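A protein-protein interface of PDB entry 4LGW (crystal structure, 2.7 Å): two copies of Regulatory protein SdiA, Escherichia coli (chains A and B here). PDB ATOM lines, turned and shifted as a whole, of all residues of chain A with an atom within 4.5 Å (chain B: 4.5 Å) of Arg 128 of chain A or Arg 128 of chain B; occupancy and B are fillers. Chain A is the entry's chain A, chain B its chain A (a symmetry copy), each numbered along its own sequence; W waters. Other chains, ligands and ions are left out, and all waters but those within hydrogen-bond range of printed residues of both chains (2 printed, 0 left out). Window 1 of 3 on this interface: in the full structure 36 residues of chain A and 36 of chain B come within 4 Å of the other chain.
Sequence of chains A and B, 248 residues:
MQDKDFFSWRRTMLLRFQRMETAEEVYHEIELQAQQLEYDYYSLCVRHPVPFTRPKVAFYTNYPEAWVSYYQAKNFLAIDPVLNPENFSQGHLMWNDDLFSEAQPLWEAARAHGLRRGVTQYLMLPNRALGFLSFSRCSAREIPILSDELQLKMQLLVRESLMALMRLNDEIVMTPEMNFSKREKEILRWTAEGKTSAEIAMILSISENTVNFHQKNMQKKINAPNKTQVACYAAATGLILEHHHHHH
SD of Met 124 of chain A sits at hydrogen-bond distance from NH1 of Arg 128 of chain B, at 3.5 Å.
The guanidinium group of Arg 128 of chain A lies within hydrogen-bond range of the side-chain sulfur of Met 124 of chain B (3.5 Å).
CE of Met 124 of chain B touches CE of Met 124 of chain A, at 3.4 Å.
Met 124 of chain A touches Leu 125 of chain B.
Leu 125 of chain A touches Met 124 of chain B (O to CE, 3.3 Å).
NE of Arg 128 of chain A touches CG of Arg 128 of chain B, 3.5 Å away.
Ala 235 of chain A touches Ala 236 of chain B.
Ala 236 of chain A touches Ala 235 of chain B.
Arg 128 of chain B touches two residues of chain A.
Of the printed residues of chain A, Leu 125 of chain B touches Met 124 (3.3 Å).
Printed residues of chain A within 4 Å of Met 124 of chain B: Met 124, Leu 125 and Arg 128.
Of the printed residues of chain B, Ala 235 of chain A touches Ala 236.
The nearest printed residue of chain B that does not touch Arg 128 of chain A is Ala 236 of chain B (5.0 Å).
The nearest printed residue of chain A that does not touch Met 124 of chain B is Pro 126 of chain A (4.1 Å).
The guanidinium group (NE) of Arg 128 of chain A lies close to the backbone carbonyl oxygen (O) of Ala 236 of chain A.
O of Ala 236 of chain B sits close to NE of Arg 128 of chain B, at 3.3 Å.
NH1 of Arg 128 of chain B sits at hydrogen-bond distance from O of Pro 126 of chain B.
The backbone carbonyl oxygen of Pro 126 of chain A is in hydrogen-bond range of the guanidinium group of Arg 128 of chain A, at 3.2 Å.
Printed residues of chain B that touch a printed residue of chain A: Met 124, Leu 125, Arg 128, Ala 235 and Ala 236.
Hydrophobic or aromatic side chains of chain B within 4 Å of the printed part of chain A: Met 124 and Ala 236.
Of the 12 printed residues of chain A, 5 touch a printed residue of chain B.
Hydrophobic or aromatic side chains of chain A within 4 Å of the printed part of chain B: Met 124 and Ala 236.
Met 124 of chain A touches its own counterpart, Met 124 of chain B.
Met 124 of chain A touches Arg 128 of chain B, and with the chains exchanged Arg 128 of chain A touches Met 124 of chain B.
Arg 128 of chain A touches its own counterpart, Arg 128 of chain B.
Ala 235 of chain A touches Ala 236 of chain B, and with the chains exchanged Ala 236 of chain A touches Ala 235 of chain B.
Positions printed for both chains: 49, 124, 125, 126, 127, 128, 129, 130, 235, 236, 237 and 238.
Of the 8 pairs that touch across the chains among the printed residues, 8 have their exchanged pair printed and touching as well.
Water W1 lies within hydrogen-bond range of the backbone carbonyl oxygen (O) of Ala 236 of chain A (2.7 Å), the guanidinium group (NH2) of Arg 128 of chain B (2.7 Å) and the backbone carbonyl oxygen (O) of Ala 235 of chain B (2.8 Å).
Water W2 lies within hydrogen-bond range of the backbone carbonyl oxygen of Ala 236 of chain B (2.7 Å), the guanidinium group of Arg 128 of chain A (2.7 Å) and the backbone carbonyl oxygen of Ala 235 of chain A (2.8 Å).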
ATOM      1  N   PRO A  49      26.499   9.617  10.387  1.00  0.00           N
ATOM      2  CA  PRO A  49      25.189   9.036  10.695  1.00  0.00           C
ATOM      3  C   PRO A  49      24.195  10.082  11.196  1.00  0.00           C
ATOM      4  O   PRO A  49      22.993   9.831  11.156  1.00  0.00           O
ATOM      5  CB  PRO A  49      25.493   8.040  11.802  1.00  0.00           C
ATOM      6  CG  PRO A  49      26.689   8.649  12.504  1.00  0.00           C
ATOM      7  CD  PRO A  49      27.506   9.301  11.421  1.00  0.00           C
ATOM      8  N   MET A 124      33.023   1.700   6.795  1.00  0.00           N
ATOM      9  CA  MET A 124      32.258   2.285   7.905  1.00  0.00           C
ATOM     10  C   MET A 124      33.223   2.394   9.065  1.00  0.00           C
ATOM     11  O   MET A 124      33.927   1.450   9.364  1.00  0.00           O
ATOM     12  CB  MET A 124      31.040   1.442   8.269  1.00  0.00           C
ATOM     13  CG  MET A 124      30.191   2.041   9.410  1.00  0.00           C
ATOM     14  SD  MET A 124      28.747   1.075   9.987  1.00  0.00           S
ATOM     15  CE  MET A 124      29.453  -0.537  10.290  1.00  0.00           C
ATOM     16  N   LEU A 125      33.277   3.561   9.686  1.00  0.00           N
ATOM     17  CA  LEU A 125      34.195   3.849  10.793  1.00  0.00           C
ATOM     18  C   LEU A 125      33.663   3.480  12.186  1.00  0.00           C
ATOM     19  O   LEU A 125      32.480   3.288  12.373  1.00  0.00           O
ATOM     20  CB  LEU A 125      34.544   5.330  10.765  1.00  0.00           C
ATOM     21  CG  LEU A 125      35.267   5.732   9.486  1.00  0.00           C
ATOM     22  CD1 LEU A 125      35.270   7.234   9.324  1.00  0.00           C
ATOM     23  CD2 LEU A 125      36.697   5.165   9.480  1.00  0.00           C
ATOM     24  N   PRO A 126      34.550   3.405  13.188  1.00  0.00           N
ATOM     25  CA  PRO A 126      34.013   3.003  14.496  1.00  0.00           C
ATOM     26  C   PRO A 126      32.869   3.880  14.978  1.00  0.00           C
ATOM     27  O   PRO A 126      32.115   3.438  15.808  1.00  0.00           O
ATOM     28  CB  PRO A 126      35.223   3.107  15.428  1.00  0.00           C
ATOM     29  CG  PRO A 126      36.401   2.869  14.480  1.00  0.00           C
ATOM     30  CD  PRO A 126      36.009   3.628  13.245  1.00  0.00           C
ATOM     31  N   ASN A 127      32.701   5.084  14.441  1.00  0.00           N
ATOM     32  CA  ASN A 127      31.622   5.956  14.900  1.00  0.00           C
ATOM     33  C   ASN A 127      30.409   5.892  13.985  1.00  0.00           C
ATOM     34  O   ASN A 127      29.540   6.769  14.050  1.00  0.00           O
ATOM     35  CB  ASN A 127      32.118   7.404  15.037  1.00  0.00           C
ATOM     36  CG  ASN A 127      32.502   8.054  13.684  1.00  0.00           C
ATOM     37  OD1 ASN A 127      32.361   7.465  12.594  1.00  0.00           O
ATOM     38  ND2 ASN A 127      32.958   9.299  13.760  1.00  0.00           N
ATOM     39  N   ARG A 128      30.391   4.889  13.100  1.00  0.00           N
ATOM     40  CA  ARG A 128      29.328   4.685  12.076  1.00  0.00           C
ATOM     41  C   ARG A 128      29.290   5.667  10.926  1.00  0.00           C
ATOM     42  O   ARG A 128      28.336   5.682  10.170  1.00  0.00           O
ATOM     43  CB  ARG A 128      27.915   4.598  12.682  1.00  0.00           C
ATOM     44  CG  ARG A 128      27.649   3.332  13.492  1.00  0.00           C
ATOM     45  CD  ARG A 128      28.426   3.355  14.800  1.00  0.00           C
ATOM     46  NE  ARG A 128      27.723   2.639  15.850  1.00  0.00           N
ATOM     47  CZ  ARG A 128      28.324   1.860  16.755  1.00  0.00           C
ATOM     48  NH1 ARG A 128      29.639   1.697  16.744  1.00  0.00           N
ATOM     49  NH2 ARG A 128      27.605   1.241  17.679  1.00  0.00           N
ATOM     50  N   ALA A 129      30.310   6.500  10.788  1.00  0.00           N
ATOM     51  CA  ALA A 129      30.373   7.375   9.628  1.00  0.00           C
ATOM     52  C   ALA A 129      30.858   6.526   8.479  1.00  0.00           C
ATOM     53  O   ALA A 129      31.680   5.628   8.672  1.00  0.00           O
ATOM     54  CB  ALA A 129      31.327   8.514   9.884  1.00  0.00           C
ATOM     55  N   LEU A 130      30.352   6.786   7.284  1.00  0.00           N
ATOM     56  CA  LEU A 130      30.885   6.122   6.099  1.00  0.00           C
ATOM     57  C   LEU A 130      31.951   6.984   5.450  1.00  0.00           C
ATOM     58  O   LEU A 130      31.707   8.144   5.120  1.00  0.00           O
ATOM     59  CB  LEU A 130      29.767   5.818   5.111  1.00  0.00           C
ATOM     60  CG  LEU A 130      28.674   4.906   5.681  1.00  0.00           C
ATOM     61  CD1 LEU A 130      27.450   4.922   4.759  1.00  0.00           C
ATOM     62  CD2 LEU A 130      29.201   3.466   5.896  1.00  0.00           C
ATOM     63  N   ALA A 235      23.104   6.354  20.464  1.00  0.00           N
ATOM     64  CA  ALA A 235      22.916   4.988  19.988  1.00  0.00           C
ATOM     65  C   ALA A 235      23.522   4.874  18.617  1.00  0.00           C
ATOM     66  O   ALA A 235      24.196   3.887  18.324  1.00  0.00           O
ATOM     67  CB  ALA A 235      21.454   4.601  19.951  1.00  0.00           C
ATOM     68  N   ALA A 236      23.311   5.904  17.794  1.00  0.00           N
ATOM     69  CA  ALA A 236      23.778   5.880  16.404  1.00  0.00           C
ATOM     70  C   ALA A 236      25.290   5.966  16.300  1.00  0.00           C
ATOM     71  O   ALA A 236      25.874   5.362  15.392  1.00  0.00           O
ATOM     72  CB  ALA A 236      23.140   6.966  15.588  1.00  0.00           C
ATOM     73  N   THR A 237      25.933   6.678  17.227  1.00  0.00           N
ATOM     74  CA  THR A 237      27.364   6.922  17.068  1.00  0.00           C
ATOM     75  C   THR A 237      28.234   6.011  17.901  1.00  0.00           C
ATOM     76  O   THR A 237      29.440   6.200  17.949  1.00  0.00           O
ATOM     77  CB  THR A 237      27.751   8.375  17.352  1.00  0.00           C
ATOM     78  OG1 THR A 237      27.456   8.681  18.716  1.00  0.00           O
ATOM     79  CG2 THR A 237      27.007   9.332  16.447  1.00  0.00           C
ATOM     80  N   GLY A 238      27.625   5.023  18.551  1.00  0.00           N
ATOM     81  CA  GLY A 238      28.341   4.124  19.436  1.00  0.00           C
ATOM     82  C   GLY A 238      28.582   4.658  20.838  1.00  0.00           C
ATOM     83  O   GLY A 238      28.991   3.904  21.723  1.00  0.00           O
ATOM     84  N   PRO B  49      24.592  -4.918  19.153  1.00  0.00           N
ATOM     85  CA  PRO B  49      24.460  -3.592  19.766  1.00  0.00           C
ATOM     86  C   PRO B  49      23.238  -3.496  20.678  1.00  0.00           C
ATOM     87  O   PRO B  49      23.188  -2.598  21.516  1.00  0.00           O
ATOM     88  CB  PRO B  49      24.288  -2.665  18.573  1.00  0.00           C
ATOM     89  CG  PRO B  49      23.612  -3.542  17.541  1.00  0.00           C
ATOM     90  CD  PRO B  49      24.194  -4.916  17.730  1.00  0.00           C
ATOM     91  N   MET B 124      33.489  -4.957  12.910  1.00  0.00           N
ATOM     92  CA  MET B 124      32.132  -4.447  13.152  1.00  0.00           C
ATOM     93  C   MET B 124      31.369  -4.660  11.864  1.00  0.00           C
ATOM     94  O   MET B 124      31.860  -4.333  10.802  1.00  0.00           O
ATOM     95  CB  MET B 124      32.136  -2.978  13.563  1.00  0.00           C
ATOM     96  CG  MET B 124      30.731  -2.414  13.859  1.00  0.00           C
ATOM     97  SD  MET B 124      30.605  -0.638  14.284  1.00  0.00           S
ATOM     98  CE  MET B 124      31.505   0.145  12.957  1.00  0.00           C
ATOM     99  N   LEU B 125      30.186  -5.245  11.962  1.00  0.00           N
ATOM    100  CA  LEU B 125      29.343  -5.572  10.808  1.00  0.00           C
ATOM    101  C   LEU B 125      28.405  -4.444  10.353  1.00  0.00           C
ATOM    102  O   LEU B 125      28.150  -3.511  11.083  1.00  0.00           O
ATOM    103  CB  LEU B 125      28.519  -6.808  11.139  1.00  0.00           C
ATOM    104  CG  LEU B 125      29.388  -8.031  11.403  1.00  0.00           C
ATOM    105  CD1 LEU B 125      28.586  -9.121  12.075  1.00  0.00           C
ATOM    106  CD2 LEU B 125      30.022  -8.529  10.091  1.00  0.00           C
ATOM    107  N   PRO B 126      27.861  -4.546   9.132  1.00  0.00           N
ATOM    108  CA  PRO B 126      27.007  -3.426   8.712  1.00  0.00           C
ATOM    109  C   PRO B 126      25.874  -3.129   9.682  1.00  0.00           C
ATOM    110  O   PRO B 126      25.367  -2.035   9.656  1.00  0.00           O
ATOM    111  CB  PRO B 126      26.468  -3.877   7.351  1.00  0.00           C
ATOM    112  CG  PRO B 126      27.568  -4.813   6.846  1.00  0.00           C
ATOM    113  CD  PRO B 126      27.965  -5.575   8.078  1.00  0.00           C
ATOM    114  N   ASN B 127      25.508  -4.057  10.559  1.00  0.00           N
ATOM    115  CA  ASN B 127      24.410  -3.806  11.488  1.00  0.00           C
ATOM    116  C   ASN B 127      24.910  -3.374  12.858  1.00  0.00           C
ATOM    117  O   ASN B 127      24.150  -3.410  13.833  1.00  0.00           O
ATOM    118  CB  ASN B 127      23.510  -5.045  11.610  1.00  0.00           C
ATOM    119  CG  ASN B 127      24.215  -6.257  12.268  1.00  0.00           C
ATOM    120  OD1 ASN B 127      25.381  -6.197  12.703  1.00  0.00           O
ATOM    121  ND2 ASN B 127      23.478  -7.357  12.371  1.00  0.00           N
ATOM    122  N   ARG B 128      26.199  -3.028  12.932  1.00  0.00           N
ATOM    123  CA  ARG B 128      26.899  -2.636  14.189  1.00  0.00           C
ATOM    124  C   ARG B 128      27.163  -3.734  15.194  1.00  0.00           C
ATOM    125  O   ARG B 128      27.543  -3.453  16.316  1.00  0.00           O
ATOM    126  CB  ARG B 128      26.214  -1.466  14.921  1.00  0.00           C
ATOM    127  CG  ARG B 128      26.325  -0.120  14.209  1.00  0.00           C
ATOM    128  CD  ARG B 128      25.465  -0.101  12.954  1.00  0.00           C
ATOM    129  NE  ARG B 128      24.969   1.234  12.670  1.00  0.00           N
ATOM    130  CZ  ARG B 128      24.877   1.750  11.439  1.00  0.00           C
ATOM    131  NH1 ARG B 128      25.242   1.047  10.379  1.00  0.00           N
ATOM    132  NH2 ARG B 128      24.414   2.980  11.269  1.00  0.00           N
ATOM    133  N   ALA B 129      26.954  -4.986  14.816  1.00  0.00           N
ATOM    134  CA  ALA B 129      27.310  -6.077  15.707  1.00  0.00           C
ATOM    135  C   ALA B 129      28.805  -6.250  15.594  1.00  0.00           C
ATOM    136  O   ALA B 129      29.372  -6.069  14.515  1.00  0.00           O
ATOM    137  CB  ALA B 129      26.599  -7.341  15.297  1.00  0.00           C
ATOM    138  N   LEU B 130      29.456  -6.585  16.695  1.00  0.00           N
ATOM    139  CA  LEU B 130      30.874  -6.927  16.637  1.00  0.00           C
ATOM    140  C   LEU B 130      31.046  -8.427  16.496  1.00  0.00           C
ATOM    141  O   LEU B 130      30.534  -9.197  17.307  1.00  0.00           O
ATOM    142  CB  LEU B 130      31.597  -6.419  17.877  1.00  0.00           C
ATOM    143  CG  LEU B 130      31.510  -4.899  18.059  1.00  0.00           C
ATOM    144  CD1 LEU B 130      31.965  -4.517  19.473  1.00  0.00           C
ATOM    145  CD2 LEU B 130      32.338  -4.157  16.981  1.00  0.00           C
ATOM    146  N   ALA B 235      18.257   3.366  15.283  1.00  0.00           N
ATOM    147  CA  ALA B 235      19.426   4.226  15.133  1.00  0.00           C
ATOM    148  C   ALA B 235      20.659   3.390  15.331  1.00  0.00           C
ATOM    149  O   ALA B 235      21.624   3.532  14.578  1.00  0.00           O
ATOM    150  CB  ALA B 235      19.407   5.376  16.115  1.00  0.00           C
ATOM    151  N   ALA B 236      20.611   2.494  16.319  1.00  0.00           N
ATOM    152  CA  ALA B 236      21.776   1.676  16.668  1.00  0.00           C
ATOM    153  C   ALA B 236      22.098   0.644  15.603  1.00  0.00           C
ATOM    154  O   ALA B 236      23.278   0.338  15.386  1.00  0.00           O
ATOM    155  CB  ALA B 236      21.604   1.008  18.001  1.00  0.00           C
ATOM    156  N   THR B 237      21.079   0.126  14.915  1.00  0.00           N
ATOM    157  CA  THR B 237      21.329  -0.985  14.002  1.00  0.00           C
ATOM    158  C   THR B 237      21.426  -0.573  12.553  1.00  0.00           C
ATOM    159  O   THR B 237      21.508  -1.427  11.682  1.00  0.00           O
ATOM    160  CB  THR B 237      20.292  -2.103  14.132  1.00  0.00           C
ATOM    161  OG1 THR B 237      19.006  -1.593  13.778  1.00  0.00           O
ATOM    162  CG2 THR B 237      20.247  -2.653  15.542  1.00  0.00           C
ATOM    163  N   GLY B 238      21.420   0.732  12.294  1.00  0.00           N
ATOM    164  CA  GLY B 238      21.440   1.251  10.940  1.00  0.00           C
ATOM    165  C   GLY B 238      20.089   1.290  10.246  1.00  0.00           C
ATOM    166  O   GLY B 238      19.959   1.900   9.183  1.00  0.00           O
HETATM  167  O   HOH W   1      24.299   3.851  13.873  1.00  0.00           O
HETATM  168  O   HOH W   2      25.061   1.742  16.772  1.00  0.00           O
